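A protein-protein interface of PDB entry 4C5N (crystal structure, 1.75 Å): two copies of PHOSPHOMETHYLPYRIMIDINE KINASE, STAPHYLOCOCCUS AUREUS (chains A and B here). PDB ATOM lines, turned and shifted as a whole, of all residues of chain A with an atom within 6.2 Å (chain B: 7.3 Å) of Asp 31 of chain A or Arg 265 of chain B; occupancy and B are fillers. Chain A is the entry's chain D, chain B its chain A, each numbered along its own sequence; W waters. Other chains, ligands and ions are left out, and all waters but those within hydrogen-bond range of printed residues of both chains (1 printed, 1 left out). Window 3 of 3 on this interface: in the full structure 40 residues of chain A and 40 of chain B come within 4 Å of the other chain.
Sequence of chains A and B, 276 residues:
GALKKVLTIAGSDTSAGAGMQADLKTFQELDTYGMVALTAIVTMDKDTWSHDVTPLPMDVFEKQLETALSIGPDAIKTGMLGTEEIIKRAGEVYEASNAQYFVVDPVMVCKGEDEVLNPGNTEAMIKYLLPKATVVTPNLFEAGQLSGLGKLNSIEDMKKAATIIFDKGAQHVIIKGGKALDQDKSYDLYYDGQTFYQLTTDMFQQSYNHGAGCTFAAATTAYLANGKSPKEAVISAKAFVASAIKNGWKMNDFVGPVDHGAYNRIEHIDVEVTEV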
ATOM      1  N   LEU A   3     -16.798 -21.341 -12.154  1.00  0.00           N
ATOM      2  CA  LEU A   3     -17.716 -20.687 -13.082  1.00  0.00           C
ATOM      3  C   LEU A   3     -18.150 -19.372 -12.492  1.00  0.00           C
ATOM      4  O   LEU A   3     -18.540 -19.326 -11.309  1.00  0.00           O
ATOM      5  CB  LEU A   3     -18.986 -21.523 -13.294  1.00  0.00           C
ATOM      6  CG  LEU A   3     -18.847 -22.836 -14.056  1.00  0.00           C
ATOM      7  CD1 LEU A   3     -20.115 -23.676 -14.108  1.00  0.00           C
ATOM      8  CD2 LEU A   3     -18.459 -22.541 -15.469  1.00  0.00           C
ATOM      9  N   LYS A   4     -18.213 -18.331 -13.322  1.00  0.00           N
ATOM     10  CA  LYS A   4     -18.758 -17.048 -12.848  1.00  0.00           C
ATOM     11  C   LYS A   4     -20.279 -17.153 -12.654  1.00  0.00           C
ATOM     12  O   LYS A   4     -20.998 -17.673 -13.513  1.00  0.00           O
ATOM     13  CB  LYS A   4     -18.343 -15.874 -13.787  1.00  0.00           C
ATOM     14  CG  LYS A   4     -16.843 -15.651 -13.985  1.00  0.00           C
ATOM     15  CD  LYS A   4     -16.168 -15.200 -12.676  1.00  0.00           C
ATOM     16  CE  LYS A   4     -14.683 -14.964 -12.892  1.00  0.00           C
ATOM     17  NZ  LYS A   4     -14.196 -14.500 -11.573  1.00  0.00           N
ATOM     18  N   THR A  26     -28.073 -18.188 -22.897  1.00  0.00           N
ATOM     19  CA  THR A  26     -26.901 -17.411 -23.305  1.00  0.00           C
ATOM     20  C   THR A  26     -25.863 -17.602 -22.277  1.00  0.00           C
ATOM     21  O   THR A  26     -24.647 -17.868 -22.594  1.00  0.00           O
ATOM     22  CB  THR A  26     -27.277 -15.951 -23.576  1.00  0.00           C
ATOM     23  OG1 THR A  26     -28.161 -15.929 -24.725  1.00  0.00           O
ATOM     24  CG2 THR A  26     -26.055 -15.156 -23.897  1.00  0.00           C
ATOM     25  N   PHE A  27     -26.253 -17.401 -21.017  1.00  0.00           N
ATOM     26  CA  PHE A  27     -25.295 -17.665 -19.950  1.00  0.00           C
ATOM     27  C   PHE A  27     -24.665 -19.092 -20.004  1.00  0.00           C
ATOM     28  O   PHE A  27     -23.456 -19.263 -19.795  1.00  0.00           O
ATOM     29  CB  PHE A  27     -25.884 -17.466 -18.575  1.00  0.00           C
ATOM     30  CG  PHE A  27     -26.460 -16.100 -18.306  1.00  0.00           C
ATOM     31  CD1 PHE A  27     -26.002 -14.936 -18.934  1.00  0.00           C
ATOM     32  CD2 PHE A  27     -27.449 -15.970 -17.332  1.00  0.00           C
ATOM     33  CE1 PHE A  27     -26.517 -13.672 -18.581  1.00  0.00           C
ATOM     34  CE2 PHE A  27     -27.936 -14.749 -16.962  1.00  0.00           C
ATOM     35  CZ  PHE A  27     -27.516 -13.580 -17.630  1.00  0.00           C
ATOM     36  N   GLN A  28     -25.488 -20.077 -20.293  1.00  0.00           N
ATOM     37  CA  GLN A  28     -25.030 -21.468 -20.386  1.00  0.00           C
ATOM     38  C   GLN A  28     -23.998 -21.601 -21.543  1.00  0.00           C
ATOM     39  O   GLN A  28     -22.915 -22.177 -21.390  1.00  0.00           O
ATOM     40  CB  GLN A  28     -26.255 -22.375 -20.521  1.00  0.00           C
ATOM     41  CG  GLN A  28     -25.945 -23.855 -20.447  1.00  0.00           C
ATOM     42  CD  GLN A  28     -25.324 -24.207 -19.134  1.00  0.00           C
ATOM     43  OE1 GLN A  28     -25.679 -23.623 -18.070  1.00  0.00           O
ATOM     44  NE2 GLN A  28     -24.424 -25.148 -19.167  1.00  0.00           N
ATOM     45  N   GLU A  29     -24.322 -20.958 -22.667  1.00  0.00           N
ATOM     46  CA  GLU A  29     -23.554 -21.055 -23.869  1.00  0.00           C
ATOM     47  C   GLU A  29     -22.226 -20.458 -23.643  1.00  0.00           C
ATOM     48  O   GLU A  29     -21.255 -20.875 -24.276  1.00  0.00           O
ATOM     49  CB  GLU A  29     -24.199 -20.357 -25.032  1.00  0.00           C
ATOM     50  CG  GLU A  29     -25.421 -21.155 -25.587  1.00  0.00           C
ATOM     51  CD  GLU A  29     -25.026 -22.363 -26.427  1.00  0.00           C
ATOM     52  OE1 GLU A  29     -23.960 -22.357 -27.017  1.00  0.00           O
ATOM     53  OE2 GLU A  29     -25.865 -23.287 -26.681  1.00  0.00           O
ATOM     54  N   LEU A  30     -22.161 -19.497 -22.759  1.00  0.00           N
ATOM     55  CA  LEU A  30     -20.971 -18.731 -22.526  1.00  0.00           C
ATOM     56  C   LEU A  30     -20.292 -19.142 -21.232  1.00  0.00           C
ATOM     57  O   LEU A  30     -19.458 -18.363 -20.732  1.00  0.00           O
ATOM     58  CB  LEU A  30     -21.136 -17.210 -22.557  1.00  0.00           C
ATOM     59  CG  LEU A  30     -21.499 -16.724 -23.926  1.00  0.00           C
ATOM     60  CD1 LEU A  30     -22.086 -15.327 -23.852  1.00  0.00           C
ATOM     61  CD2 LEU A  30     -20.321 -16.801 -24.921  1.00  0.00           C
ATOM     62  N   ASP A  31     -20.515 -20.378 -20.807  1.00  0.00           N
ATOM     63  CA  ASP A  31     -19.655 -20.972 -19.749  1.00  0.00           C
ATOM     64  C   ASP A  31     -19.638 -20.175 -18.452  1.00  0.00           C
ATOM     65  O   ASP A  31     -18.602 -19.979 -17.790  1.00  0.00           O
ATOM     66  CB  ASP A  31     -18.244 -21.329 -20.234  1.00  0.00           C
ATOM     67  CG  ASP A  31     -18.254 -22.231 -21.480  1.00  0.00           C
ATOM     68  OD1 ASP A  31     -19.231 -23.019 -21.724  1.00  0.00           O
ATOM     69  OD2 ASP A  31     -17.253 -22.136 -22.219  1.00  0.00           O
ATOM     70  N   THR A  32     -20.843 -19.749 -18.070  1.00  0.00           N
ATOM     71  CA  THR A  32     -21.076 -19.108 -16.762  1.00  0.00           C
ATOM     72  C   THR A  32     -22.180 -19.913 -16.093  1.00  0.00           C
ATOM     73  O   THR A  32     -22.921 -20.683 -16.779  1.00  0.00           O
ATOM     74  CB  THR A  32     -21.503 -17.623 -16.879  1.00  0.00           C
ATOM     75  OG1 THR A  32     -22.738 -17.532 -17.602  1.00  0.00           O
ATOM     76  CG2 THR A  32     -20.464 -16.875 -17.658  1.00  0.00           C
ATOM     77  N   TYR A  33     -22.365 -19.665 -14.800  1.00  0.00           N
ATOM     78  CA  TYR A  33     -23.465 -20.297 -14.014  1.00  0.00           C
ATOM     79  C   TYR A  33     -24.622 -19.315 -13.941  1.00  0.00           C
ATOM     80  O   TYR A  33     -24.578 -18.300 -13.254  1.00  0.00           O
ATOM     81  CB  TYR A  33     -22.977 -20.619 -12.614  1.00  0.00           C
ATOM     82  CG  TYR A  33     -23.998 -21.321 -11.761  1.00  0.00           C
ATOM     83  CD1 TYR A  33     -24.242 -22.681 -11.903  1.00  0.00           C
ATOM     84  CD2 TYR A  33     -24.758 -20.619 -10.847  1.00  0.00           C
ATOM     85  CE1 TYR A  33     -25.162 -23.368 -11.112  1.00  0.00           C
ATOM     86  CE2 TYR A  33     -25.695 -21.283 -10.037  1.00  0.00           C
ATOM     87  CZ  TYR A  33     -25.943 -22.660 -10.199  1.00  0.00           C
ATOM     88  OH  TYR A  33     -26.859 -23.348  -9.369  1.00  0.00           O
ATOM     89  N   ASN A 226     -16.557 -12.943 -17.410  1.00  0.00           N
ATOM     90  CA  ASN A 226     -15.443 -13.769 -17.837  1.00  0.00           C
ATOM     91  C   ASN A 226     -14.150 -12.953 -18.153  1.00  0.00           C
ATOM     92  O   ASN A 226     -13.105 -13.565 -18.502  1.00  0.00           O
ATOM     93  CB  ASN A 226     -15.924 -14.624 -19.032  1.00  0.00           C
ATOM     94  CG  ASN A 226     -16.747 -15.818 -18.622  1.00  0.00           C
ATOM     95  OD1 ASN A 226     -16.663 -16.295 -17.497  1.00  0.00           O
ATOM     96  ND2 ASN A 226     -17.538 -16.319 -19.536  1.00  0.00           N
ATOM     97  N   ASN A 264     -21.639 -20.829 -30.976  1.00  0.00           N
ATOM     98  CA  ASN A 264     -20.793 -22.018 -30.627  1.00  0.00           C
ATOM     99  C   ASN A 264     -20.969 -23.259 -31.501  1.00  0.00           C
ATOM    100  O   ASN A 264     -19.996 -23.967 -31.657  1.00  0.00           O
ATOM    101  CB  ASN A 264     -20.945 -22.417 -29.158  1.00  0.00           C
ATOM    102  CG  ASN A 264     -20.456 -21.359 -28.233  1.00  0.00           C
ATOM    103  OD1 ASN A 264     -19.514 -20.591 -28.553  1.00  0.00           O
ATOM    104  ND2 ASN A 264     -21.066 -21.311 -27.086  1.00  0.00           N
ATOM    105  N   GLU B  29     -27.527 -27.435 -23.749  1.00  0.00           N
ATOM    106  CA  GLU B  29     -26.321 -28.171 -23.915  1.00  0.00           C
ATOM    107  C   GLU B  29     -26.495 -29.247 -24.924  1.00  0.00           C
ATOM    108  O   GLU B  29     -25.522 -29.625 -25.644  1.00  0.00           O
ATOM    109  CB  GLU B  29     -25.779 -28.720 -22.575  1.00  0.00           C
ATOM    110  CG  GLU B  29     -25.210 -27.630 -21.645  1.00  0.00           C
ATOM    111  CD  GLU B  29     -23.798 -27.160 -22.019  1.00  0.00           C
ATOM    112  OE1 GLU B  29     -23.033 -27.887 -22.698  1.00  0.00           O
ATOM    113  OE2 GLU B  29     -23.410 -26.054 -21.588  1.00  0.00           O
ATOM    114  N   SER B 243     -20.594 -36.716 -15.820  1.00  0.00           N
ATOM    115  CA  SER B 243     -19.602 -35.651 -15.986  1.00  0.00           C
ATOM    116  C   SER B 243     -19.995 -34.429 -15.119  1.00  0.00           C
ATOM    117  O   SER B 243     -19.180 -33.799 -14.482  1.00  0.00           O
ATOM    118  CB  SER B 243     -19.528 -35.275 -17.480  1.00  0.00           C
ATOM    119  OG  SER B 243     -18.519 -34.254 -17.667  1.00  0.00           O
ATOM    120  N   ASN B 247     -17.822 -32.984 -11.951  1.00  0.00           N
ATOM    121  CA  ASN B 247     -17.365 -31.611 -11.956  1.00  0.00           C
ATOM    122  C   ASN B 247     -18.189 -30.630 -11.137  1.00  0.00           C
ATOM    123  O   ASN B 247     -18.198 -29.400 -11.416  1.00  0.00           O
ATOM    124  CB  ASN B 247     -17.175 -31.185 -13.425  1.00  0.00           C
ATOM    125  CG  ASN B 247     -16.036 -31.965 -14.116  1.00  0.00           C
ATOM    126  OD1 ASN B 247     -14.888 -31.653 -13.897  1.00  0.00           O
ATOM    127  ND2 ASN B 247     -16.364 -32.972 -14.960  1.00  0.00           N
ATOM    128  N   ASP B 259     -22.161 -29.454 -12.606  1.00  0.00           N
ATOM    129  CA  ASP B 259     -21.839 -28.618 -13.725  1.00  0.00           C
ATOM    130  C   ASP B 259     -22.487 -29.080 -15.046  1.00  0.00           C
ATOM    131  O   ASP B 259     -21.963 -29.986 -15.759  1.00  0.00           O
ATOM    132  CB  ASP B 259     -20.340 -28.478 -13.806  1.00  0.00           C
ATOM    133  CG  ASP B 259     -19.867 -27.580 -14.945  1.00  0.00           C
ATOM    134  OD1 ASP B 259     -20.634 -27.150 -15.805  1.00  0.00           O
ATOM    135  OD2 ASP B 259     -18.659 -27.288 -14.915  1.00  0.00           O
ATOM    136  N   HIS B 260     -23.665 -28.497 -15.363  1.00  0.00           N
ATOM    137  CA  HIS B 260     -24.489 -29.034 -16.436  1.00  0.00           C
ATOM    138  C   HIS B 260     -23.742 -29.036 -17.791  1.00  0.00           C
ATOM    139  O   HIS B 260     -24.070 -29.822 -18.681  1.00  0.00           O
ATOM    140  CB  HIS B 260     -25.841 -28.329 -16.595  1.00  0.00           C
ATOM    141  CG  HIS B 260     -26.533 -28.009 -15.294  1.00  0.00           C
ATOM    142  ND1 HIS B 260     -26.126 -26.981 -14.462  1.00  0.00           N
ATOM    143  CD2 HIS B 260     -27.567 -28.617 -14.656  1.00  0.00           C
ATOM    144  CE1 HIS B 260     -26.842 -26.999 -13.353  1.00  0.00           C
ATOM    145  NE2 HIS B 260     -27.710 -27.990 -13.434  1.00  0.00           N
ATOM    146  N   GLY B 261     -22.790 -28.125 -17.944  1.00  0.00           N
ATOM    147  CA  GLY B 261     -22.011 -28.004 -19.173  1.00  0.00           C
ATOM    148  C   GLY B 261     -20.755 -28.883 -19.227  1.00  0.00           C
ATOM    149  O   GLY B 261     -20.007 -28.802 -20.210  1.00  0.00           O
ATOM    150  N   ALA B 262     -20.522 -29.736 -18.243  1.00  0.00           N
ATOM    151  CA  ALA B 262     -19.213 -30.469 -18.151  1.00  0.00           C
ATOM    152  C   ALA B 262     -18.992 -31.485 -19.218  1.00  0.00           C
ATOM    153  O   ALA B 262     -17.870 -31.678 -19.663  1.00  0.00           O
ATOM    154  CB  ALA B 262     -19.070 -31.135 -16.755  1.00  0.00           C
ATOM    155  N   TYR B 263     -20.062 -32.140 -19.637  1.00  0.00           N
ATOM    156  CA  TYR B 263     -19.959 -33.234 -20.640  1.00  0.00           C
ATOM    157  C   TYR B 263     -19.383 -32.667 -21.933  1.00  0.00           C
ATOM    158  O   TYR B 263     -18.435 -33.225 -22.489  1.00  0.00           O
ATOM    159  CB  TYR B 263     -21.301 -33.904 -20.870  1.00  0.00           C
ATOM    160  CG  TYR B 263     -21.300 -35.034 -21.906  1.00  0.00           C
ATOM    161  CD1 TYR B 263     -20.912 -36.348 -21.572  1.00  0.00           C
ATOM    162  CD2 TYR B 263     -21.679 -34.770 -23.234  1.00  0.00           C
ATOM    163  CE1 TYR B 263     -20.882 -37.369 -22.510  1.00  0.00           C
ATOM    164  CE2 TYR B 263     -21.680 -35.782 -24.171  1.00  0.00           C
ATOM    165  CZ  TYR B 263     -21.234 -37.075 -23.818  1.00  0.00           C
ATOM    166  OH  TYR B 263     -21.263 -38.102 -24.751  1.00  0.00           O
ATOM    167  N   ASN B 264     -19.874 -31.494 -22.345  1.00  0.00           N
ATOM    168  CA  ASN B 264     -19.394 -30.876 -23.549  1.00  0.00           C
ATOM    169  C   ASN B 264     -18.158 -30.063 -23.312  1.00  0.00           C
ATOM    170  O   ASN B 264     -17.333 -29.938 -24.221  1.00  0.00           O
ATOM    171  CB  ASN B 264     -20.440 -29.937 -24.174  1.00  0.00           C
ATOM    172  CG  ASN B 264     -21.594 -30.698 -24.755  1.00  0.00           C
ATOM    173  OD1 ASN B 264     -21.415 -31.810 -25.252  1.00  0.00           O
ATOM    174  ND2 ASN B 264     -22.796 -30.100 -24.734  1.00  0.00           N
ATOM    175  N   ARG B 265     -18.000 -29.488 -22.135  1.00  0.00           N
ATOM    176  CA  ARG B 265     -16.819 -28.555 -21.962  1.00  0.00           C
ATOM    177  C   ARG B 265     -15.570 -29.239 -21.360  1.00  0.00           C
ATOM    178  O   ARG B 265     -14.443 -28.802 -21.640  1.00  0.00           O
ATOM    179  CB  ARG B 265     -17.190 -27.327 -21.142  1.00  0.00           C
ATOM    180  CG  ARG B 265     -16.112 -26.236 -21.070  1.00  0.00           C
ATOM    181  CD  ARG B 265     -16.472 -24.976 -20.304  1.00  0.00           C
ATOM    182  NE  ARG B 265     -17.268 -25.288 -19.157  1.00  0.00           N
ATOM    183  CZ  ARG B 265     -16.796 -25.775 -18.020  1.00  0.00           C
ATOM    184  NH1 ARG B 265     -15.489 -25.948 -17.821  1.00  0.00           N
ATOM    185  NH2 ARG B 265     -17.630 -26.081 -17.076  1.00  0.00           N
ATOM    186  N   ILE B 266     -15.765 -30.272 -20.536  1.00  0.00           N
ATOM    187  CA  ILE B 266     -14.649 -30.847 -19.781  1.00  0.00           C
ATOM    188  C   ILE B 266     -14.375 -32.269 -20.263  1.00  0.00           C
ATOM    189  O   ILE B 266     -13.290 -32.570 -20.750  1.00  0.00           O
ATOM    190  CB  ILE B 266     -14.966 -30.796 -18.281  1.00  0.00           C
ATOM    191  CG1 ILE B 266     -15.312 -29.377 -17.865  1.00  0.00           C
ATOM    192  CG2 ILE B 266     -13.794 -31.325 -17.394  1.00  0.00           C
ATOM    193  CD1 ILE B 266     -15.761 -29.278 -16.419  1.00  0.00           C
ATOM    194  N   GLU B 267     -15.361 -33.152 -20.220  1.00  0.00           N
ATOM    195  CA  GLU B 267     -15.052 -34.573 -20.457  1.00  0.00           C
ATOM    196  C   GLU B 267     -16.291 -35.385 -20.572  1.00  0.00           C
ATOM    197  O   GLU B 267     -17.363 -35.073 -19.938  1.00  0.00           O
ATOM    198  CB  GLU B 267     -14.203 -35.115 -19.284  1.00  0.00           C
ATOM    199  CG  GLU B 267     -14.979 -35.308 -18.001  1.00  0.00           C
ATOM    200  CD  GLU B 267     -14.069 -35.462 -16.783  1.00  0.00           C
ATOM    201  OE1 GLU B 267     -13.269 -36.441 -16.725  1.00  0.00           O
ATOM    202  OE2 GLU B 267     -14.114 -34.587 -15.898  1.00  0.00           O
ATOM    203  N   HIS B 268     -16.181 -36.435 -21.387  1.00  0.00           N
ATOM    204  CA  HIS B 268     -17.165 -37.484 -21.376  1.00  0.00           C
ATOM    205  C   HIS B 268     -16.852 -38.485 -20.286  1.00  0.00           C
ATOM    206  O   HIS B 268     -15.707 -38.571 -19.880  1.00  0.00           O
ATOM    207  CB  HIS B 268     -17.147 -38.199 -22.726  1.00  0.00           C
ATOM    208  CG  HIS B 268     -17.621 -37.346 -23.850  1.00  0.00           C
ATOM    209  ND1 HIS B 268     -17.906 -37.852 -25.098  1.00  0.00           N
ATOM    210  CD2 HIS B 268     -17.898 -36.015 -23.908  1.00  0.00           C
ATOM    211  CE1 HIS B 268     -18.310 -36.868 -25.885  1.00  0.00           C
ATOM    212  NE2 HIS B 268     -18.339 -35.749 -25.179  1.00  0.00           N
HETATM  213  O   HOH W   1     -22.529 -25.290 -16.736  1.00  0.00           O
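2 positions are printed for both chains.
Water W1 lies within hydrogen-bond range of the side-chain carboxylate of Asp 259 of chain B (2.8 Å), the side-chain amide nitrogen of Gln 28 of chain A (3.1 Å) and the backbone NH of Gly 261 of chain B (3.1 Å).
Printed residues of chain A that touch a printed residue of chain B: Leu 3, Gln 28 and Asp 31.
Along chain A the printed residues that touch a printed residue of chain B span positions 3 to 31.
Among the printed residues, 5 pairs touch across the chains.
Leu 3 of chain A touches Asp 259 of chain B (CD1 to OD1, 3.9 Å).
Leu 3 of chain A touches Arg 265 of chain B (CD2 to NH2, 3.98 Å).
N of Gly 261 of chain B touches NE2 of Gln 28 of chain A (3.6 Å).
The guanidinium group of Arg 265 of chain B is in salt-bridge range of the side-chain carboxylate of Asp 259 of chain B, 2.7 Å away.
The side-chain carboxylate of Asp 259 of chain B sits close to the backbone NH of Gly 261 of chain B (3.2 Å).
The side-chain amide nitrogen (ND2) of Asn 264 of chain B is in hydrogen-bond range of the backbone carbonyl oxygen (O) of Glu 29 of chain B, 2.9 Å away.
The side-chain carboxylate (OD1) of Asp 31 of chain A is in salt-bridge range of the guanidinium group (NE) of Arg 265 of chain B, 3.9 Å away.
NE2 of Gln 28 of chain A sits at hydrogen-bond distance from OE2 of Glu 29 of chain B (2.8 Å).
Of the printed residues of chain B, Asp 31 of chain A touches Arg 265.
Of chain A, only Leu 3 (3.98 Å) and Asp 31 (3.5 Å) come within 4 Å of Arg 265 of chain B.
Printed residues of chain A within 4 Å of Asp 259 of chain B: Leu 3.
Of the printed residues of chain A, Gly 261 of chain B touches Gln 28 (3.6 Å).
Printed residues of chain B within 4 Å of Leu 3 of chain A: Asp 259 and Arg 265.
Printed residues of chain A within 4 Å of Glu 29 of chain B: Gln 28.
Printed residues of chain B within 4 Å of Gln 28 of chain A: Glu 29 and Gly 261.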
